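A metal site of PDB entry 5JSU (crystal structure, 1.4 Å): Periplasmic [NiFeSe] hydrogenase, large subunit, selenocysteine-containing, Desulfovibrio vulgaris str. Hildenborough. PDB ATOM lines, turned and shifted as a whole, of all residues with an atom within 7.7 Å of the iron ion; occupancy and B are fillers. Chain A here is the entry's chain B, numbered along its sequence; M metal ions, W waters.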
ATOM      1  N   GLU A  53     -30.574  18.993  23.681  1.00  0.00           N
ATOM      2  CA  GLU A  53     -29.985  20.257  23.276  1.00  0.00           C
ATOM      3  C   GLU A  53     -29.682  20.309  21.780  1.00  0.00           C
ATOM      4  O   GLU A  53     -29.685  21.394  21.195  1.00  0.00           O
ATOM      5  CB  GLU A  53     -28.749  20.557  24.112  1.00  0.00           C
ATOM      6  CG  GLU A  53     -29.109  20.828  25.590  1.00  0.00           C
ATOM      7  CD  GLU A  53     -27.994  20.514  26.573  1.00  0.00           C
ATOM      8  OE1 GLU A  53     -27.164  19.635  26.297  1.00  0.00           O
ATOM      9  OE2 GLU A  53     -27.992  21.137  27.672  1.00  0.00           O
ATOM     10  N   GLU A 279     -19.503  24.427  32.706  1.00  0.00           N
ATOM     11  CA  GLU A 279     -19.680  22.983  32.635  1.00  0.00           C
ATOM     12  C   GLU A 279     -18.429  22.317  32.066  1.00  0.00           C
ATOM     13  O   GLU A 279     -18.038  22.577  30.921  1.00  0.00           O
ATOM     14  CB  GLU A 279     -20.906  22.616  31.805  1.00  0.00           C
ATOM     15  CG  GLU A 279     -22.223  23.032  32.474  1.00  0.00           C
ATOM     16  CD  GLU A 279     -23.427  22.460  31.740  1.00  0.00           C
ATOM     17  OE1 GLU A 279     -23.817  23.035  30.705  1.00  0.00           O
ATOM     18  OE2 GLU A 279     -23.983  21.445  32.196  1.00  0.00           O
ATOM     19  N   PHE A 286     -18.231  13.744  26.346  1.00  0.00           N
ATOM     20  CA  PHE A 286     -18.376  14.849  25.404  1.00  0.00           C
ATOM     21  C   PHE A 286     -17.018  15.300  24.902  1.00  0.00           C
ATOM     22  O   PHE A 286     -15.987  15.078  25.546  1.00  0.00           O
ATOM     23  CB  PHE A 286     -19.148  16.024  26.027  1.00  0.00           C
ATOM     24  CG  PHE A 286     -20.513  15.626  26.468  1.00  0.00           C
ATOM     25  CD1 PHE A 286     -21.528  15.507  25.542  1.00  0.00           C
ATOM     26  CD2 PHE A 286     -20.766  15.265  27.777  1.00  0.00           C
ATOM     27  CE1 PHE A 286     -22.783  15.079  25.916  1.00  0.00           C
ATOM     28  CE2 PHE A 286     -22.016  14.828  28.161  1.00  0.00           C
ATOM     29  CZ  PHE A 286     -23.030  14.723  27.238  1.00  0.00           C
ATOM     30  N   TYR A 295     -23.183  28.321  30.088  1.00  0.00           N
ATOM     31  CA  TYR A 295     -24.321  27.807  29.331  1.00  0.00           C
ATOM     32  C   TYR A 295     -24.709  28.720  28.167  1.00  0.00           C
ATOM     33  O   TYR A 295     -25.253  28.227  27.167  1.00  0.00           O
ATOM     34  CB  TYR A 295     -25.522  27.525  30.257  1.00  0.00           C
ATOM     35  CG  TYR A 295     -25.949  28.780  31.004  1.00  0.00           C
ATOM     36  CD1 TYR A 295     -26.790  29.714  30.416  1.00  0.00           C
ATOM     37  CD2 TYR A 295     -25.450  29.057  32.273  1.00  0.00           C
ATOM     38  CE1 TYR A 295     -27.125  30.880  31.070  1.00  0.00           C
ATOM     39  CE2 TYR A 295     -25.770  30.223  32.919  1.00  0.00           C
ATOM     40  CZ  TYR A 295     -26.609  31.137  32.322  1.00  0.00           C
ATOM     41  OH  TYR A 295     -26.944  32.299  32.951  1.00  0.00           O
ATOM     42  N   LYS A 299     -22.179  23.852  24.510  1.00  0.00           N
ATOM     43  CA  LYS A 299     -22.106  22.959  23.364  1.00  0.00           C
ATOM     44  C   LYS A 299     -22.282  21.535  23.847  1.00  0.00           C
ATOM     45  O   LYS A 299     -21.836  21.183  24.950  1.00  0.00           O
ATOM     46  CB  LYS A 299     -20.751  23.051  22.657  1.00  0.00           C
ATOM     47  CG  LYS A 299     -20.457  24.408  22.059  1.00  0.00           C
ATOM     48  CD  LYS A 299     -19.235  24.359  21.172  1.00  0.00           C
ATOM     49  CE  LYS A 299     -19.069  25.625  20.355  1.00  0.00           C
ATOM     50  NZ  LYS A 299     -20.246  25.868  19.474  1.00  0.00           N
ATOM     51  N   THR A 300     -22.936  20.715  23.033  1.00  0.00           N
ATOM     52  CA  THR A 300     -23.244  19.339  23.411  1.00  0.00           C
ATOM     53  C   THR A 300     -22.869  18.431  22.248  1.00  0.00           C
ATOM     54  O   THR A 300     -23.630  18.252  21.297  1.00  0.00           O
ATOM     55  CB  THR A 300     -24.694  19.226  23.813  1.00  0.00           C
ATOM     56  OG1 THR A 300     -24.905  20.147  24.881  1.00  0.00           O
ATOM     57  CG2 THR A 300     -25.022  17.803  24.304  1.00  0.00           C
ATOM     58  N   PHE A 312     -22.510  10.470  31.102  1.00  0.00           N
ATOM     59  CA  PHE A 312     -23.132  11.406  30.180  1.00  0.00           C
ATOM     60  C   PHE A 312     -23.591  12.702  30.867  1.00  0.00           C
ATOM     61  O   PHE A 312     -24.136  13.583  30.196  1.00  0.00           O
ATOM     62  CB  PHE A 312     -24.315  10.778  29.432  1.00  0.00           C
ATOM     63  CG  PHE A 312     -23.915   9.769  28.390  1.00  0.00           C
ATOM     64  CD1 PHE A 312     -23.208  10.158  27.263  1.00  0.00           C
ATOM     65  CD2 PHE A 312     -24.274   8.430  28.527  1.00  0.00           C
ATOM     66  CE1 PHE A 312     -22.844   9.239  26.295  1.00  0.00           C
ATOM     67  CE2 PHE A 312     -23.910   7.511  27.559  1.00  0.00           C
ATOM     68  CZ  PHE A 312     -23.206   7.906  26.439  1.00  0.00           C
ATOM     69  N   LYS A 314     -22.613  16.185  32.389  1.00  0.00           N
ATOM     70  CA  LYS A 314     -21.532  17.161  32.443  1.00  0.00           C
ATOM     71  C   LYS A 314     -21.250  17.517  33.914  1.00  0.00           C
ATOM     72  O   LYS A 314     -22.000  17.133  34.816  1.00  0.00           O
ATOM     73  CB  LYS A 314     -21.899  18.429  31.672  1.00  0.00           C
ATOM     74  CG  LYS A 314     -22.069  18.269  30.151  1.00  0.00           C
ATOM     75  CD  LYS A 314     -22.435  19.574  29.498  1.00  0.00           C
ATOM     76  CE  LYS A 314     -22.628  19.429  27.983  1.00  0.00           C
ATOM     77  NZ  LYS A 314     -23.248  20.675  27.429  1.00  0.00           N
ATOM     78  N   LEU A 423     -32.048  25.783  34.992  1.00  0.00           N
ATOM     79  CA  LEU A 423     -32.090  26.889  34.048  1.00  0.00           C
ATOM     80  C   LEU A 423     -32.083  26.380  32.614  1.00  0.00           C
ATOM     81  O   LEU A 423     -31.500  25.328  32.303  1.00  0.00           O
ATOM     82  CB  LEU A 423     -30.978  27.923  34.257  1.00  0.00           C
ATOM     83  CG  LEU A 423     -29.561  27.474  33.911  1.00  0.00           C
ATOM     84  CD1 LEU A 423     -29.228  27.763  32.449  1.00  0.00           C
ATOM     85  CD2 LEU A 423     -28.546  28.131  34.839  1.00  0.00           C
ATOM     86  N   TYR A 436     -29.858  25.784  22.437  1.00  0.00           N
ATOM     87  CA  TYR A 436     -30.676  25.597  23.637  1.00  0.00           C
ATOM     88  C   TYR A 436     -29.821  24.817  24.618  1.00  0.00           C
ATOM     89  O   TYR A 436     -29.339  23.730  24.295  1.00  0.00           O
ATOM     90  CB  TYR A 436     -31.957  24.849  23.289  1.00  0.00           C
ATOM     91  CG  TYR A 436     -33.082  25.069  24.277  1.00  0.00           C
ATOM     92  CD1 TYR A 436     -33.073  24.477  25.541  1.00  0.00           C
ATOM     93  CD2 TYR A 436     -34.174  25.874  23.941  1.00  0.00           C
ATOM     94  CE1 TYR A 436     -34.119  24.680  26.439  1.00  0.00           C
ATOM     95  CE2 TYR A 436     -35.215  26.064  24.824  1.00  0.00           C
ATOM     96  CZ  TYR A 436     -35.181  25.469  26.061  1.00  0.00           C
ATOM     97  OH  TYR A 436     -36.244  25.701  26.913  1.00  0.00           O
ATOM     98  N   GLN A 437     -29.588  25.384  25.801  1.00  0.00           N
ATOM     99  CA  GLN A 437     -28.734  24.744  26.800  1.00  0.00           C
ATOM    100  C   GLN A 437     -29.471  24.625  28.127  1.00  0.00           C
ATOM    101  O   GLN A 437     -30.130  25.571  28.576  1.00  0.00           O
ATOM    102  CB  GLN A 437     -27.403  25.493  26.965  1.00  0.00           C
ATOM    103  CG  GLN A 437     -26.452  25.286  25.789  1.00  0.00           C
ATOM    104  CD  GLN A 437     -25.898  23.878  25.719  1.00  0.00           C
ATOM    105  OE1 GLN A 437     -25.493  23.321  26.732  1.00  0.00           O
ATOM    106  NE2 GLN A 437     -25.866  23.292  24.522  1.00  0.00           N
ATOM    107  N   ILE A 438     -29.348  23.449  28.739  1.00  0.00           N
ATOM    108  CA  ILE A 438     -30.080  23.098  29.947  1.00  0.00           C
ATOM    109  C   ILE A 438     -29.088  22.735  31.044  1.00  0.00           C
ATOM    110  O   ILE A 438     -28.161  21.935  30.822  1.00  0.00           O
ATOM    111  CB  ILE A 438     -31.050  21.938  29.668  1.00  0.00           C
ATOM    112  CG1 ILE A 438     -32.088  22.442  28.680  1.00  0.00           C
ATOM    113  CG2 ILE A 438     -31.695  21.398  30.985  1.00  0.00           C
ATOM    114  CD1 ILE A 438     -32.812  21.392  27.934  1.00  0.00           C
ATOM    115  N   VAL A 439     -29.259  23.343  32.209  1.00  0.00           N
ATOM    116  CA  VAL A 439     -28.439  23.072  33.380  1.00  0.00           C
ATOM    117  C   VAL A 439     -29.449  22.742  34.473  1.00  0.00           C
ATOM    118  O   VAL A 439     -30.133  23.631  34.975  1.00  0.00           O
ATOM    119  CB  VAL A 439     -27.555  24.265  33.746  1.00  0.00           C
ATOM    120  CG1 VAL A 439     -26.732  23.990  34.975  1.00  0.00           C
ATOM    121  CG2 VAL A 439     -26.614  24.643  32.558  1.00  0.00           C
ATOM    122  N   SER A 440     -29.574  21.456  34.808  1.00  0.00           N
ATOM    123  CA  SER A 440     -30.691  20.928  35.590  1.00  0.00           C
ATOM    124  C   SER A 440     -30.268  20.516  37.005  1.00  0.00           C
ATOM    125  O   SER A 440     -29.089  20.497  37.376  1.00  0.00           O
ATOM    126  CB  SER A 440     -31.271  19.738  34.854  1.00  0.00           C
ATOM    127  OG  SER A 440     -30.250  18.753  34.794  1.00  0.00           O
ATOM    128  N   LEU A 443     -28.212  17.252  37.474  1.00  0.00           N
ATOM    129  CA  LEU A 443     -26.906  17.588  36.952  1.00  0.00           C
ATOM    130  C   LEU A 443     -25.992  18.113  38.058  1.00  0.00           C
ATOM    131  O   LEU A 443     -24.845  17.680  38.176  1.00  0.00           O
ATOM    132  CB  LEU A 443     -27.064  18.615  35.839  1.00  0.00           C
ATOM    133  CG  LEU A 443     -25.833  19.375  35.385  1.00  0.00           C
ATOM    134  CD1 LEU A 443     -24.903  18.456  34.640  1.00  0.00           C
ATOM    135  CD2 LEU A 443     -26.224  20.562  34.549  1.00  0.00           C
ATOM    136  N   CYS A 489     -33.129  14.023  33.783  1.00  0.00           N
ATOM    137  CA  CYS A 489     -32.802  15.442  33.907  1.00  0.00           C
ATOM    138  C   CYS A 489     -31.303  15.687  33.889  1.00  0.00           C
ATOM    139  O   CYS A 489     -30.826  16.660  33.287  1.00  0.00           O
ATOM    140  CB  CYS A 489     -33.371  15.995  35.191  1.00  0.00           C
ATOM    141  SG  CYS A 489     -35.114  16.257  35.101  1.00  0.00           S
ATOM    142  N   ALA A 490     -30.545  14.841  34.574  1.00  0.00           N
ATOM    143  CA  ALA A 490     -29.128  15.116  34.701  1.00  0.00           C
ATOM    144  C   ALA A 490     -28.429  15.121  33.347  1.00  0.00           C
ATOM    145  O   ALA A 490     -27.520  15.933  33.116  1.00  0.00           O
ATOM    146  CB  ALA A 490     -28.476  14.092  35.628  1.00  0.00           C
ATOM    147  N   VAL A 491     -28.822  14.221  32.444  1.00  0.00           N
ATOM    148  CA  VAL A 491     -28.166  14.053  31.147  1.00  0.00           C
ATOM    149  C   VAL A 491     -28.906  14.804  30.046  1.00  0.00           C
ATOM    150  O   VAL A 491     -28.271  15.393  29.160  1.00  0.00           O
ATOM    151  CB  VAL A 491     -28.053  12.567  30.765  1.00  0.00           C
ATOM    152  CG1 VAL A 491     -27.436  12.438  29.380  1.00  0.00           C
ATOM    153  CG2 VAL A 491     -27.258  11.783  31.794  1.00  0.00           C
ATOM    154  N   HIS A 492     -30.230  14.695  30.008  1.00  0.00           N
ATOM    155  CA  HIS A 492     -31.053  15.191  28.908  1.00  0.00           C
ATOM    156  C   HIS A 492     -30.492  14.863  27.529  1.00  0.00           C
ATOM    157  O   HIS A 492     -30.135  13.686  27.313  1.00  0.00           O
ATOM    158  CB  HIS A 492     -31.390  16.693  29.066  1.00  0.00           C
ATOM    159  CG  HIS A 492     -30.271  17.565  29.546  1.00  0.00           C
ATOM    160  ND1 HIS A 492     -29.881  17.609  30.870  1.00  0.00           N
ATOM    161  CD2 HIS A 492     -29.466  18.441  28.897  1.00  0.00           C
ATOM    162  CE1 HIS A 492     -28.884  18.461  31.007  1.00  0.00           C
ATOM    163  NE2 HIS A 492     -28.616  18.986  29.825  1.00  0.00           N
HETATM  164 FE    FE M   1     -27.009  20.492  29.540  1.00  0.00          FE
HETATM  165  O   HOH W   1     -25.493  22.005  29.038  1.00  0.00           O
HETATM  166  O   HOH W   2     -25.783  18.959  28.375  1.00  0.00           O
HETATM  167  O   HOH W   3     -25.879  19.894  31.292  1.00  0.00           O
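Water W1 lies within hydrogen-bond range of OE1 of Glu 279, OE1 of Gln 437 and NZ of Lys 314. Water W2 lies within hydrogen-bond range of the side-chain carboxylate of Glu 53 and the side-chain amino group of Lys 314.
Within 4 Å of the iron ion: Glu 53, Ile 438 and His 492.
The side-chain carboxylate (OE2) of Glu 53 lies close to the side-chain amide oxygen (OE1) of Gln 437. OE1 of Glu 53 sits at hydrogen-bond distance from OG1 of Thr 300 (2.7 Å). The backbone carbonyl oxygen of Cys 489 lies within hydrogen-bond range of a ring nitrogen (ND1) of His 492 (2.8 Å).
The iron ion is bound by water W3, 2.2 Å away. The iron ion is bound by water W1, at 2.2 Å. The side-chain carboxylate (OE2) of Glu 53 is bound to the iron ion (2.2 Å). The iron ion is bound by NE2 of His 492. The iron ion is bound by O of Ile 438 (2.2 Å). The iron ion is bound by water W2 (2.3 Å).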
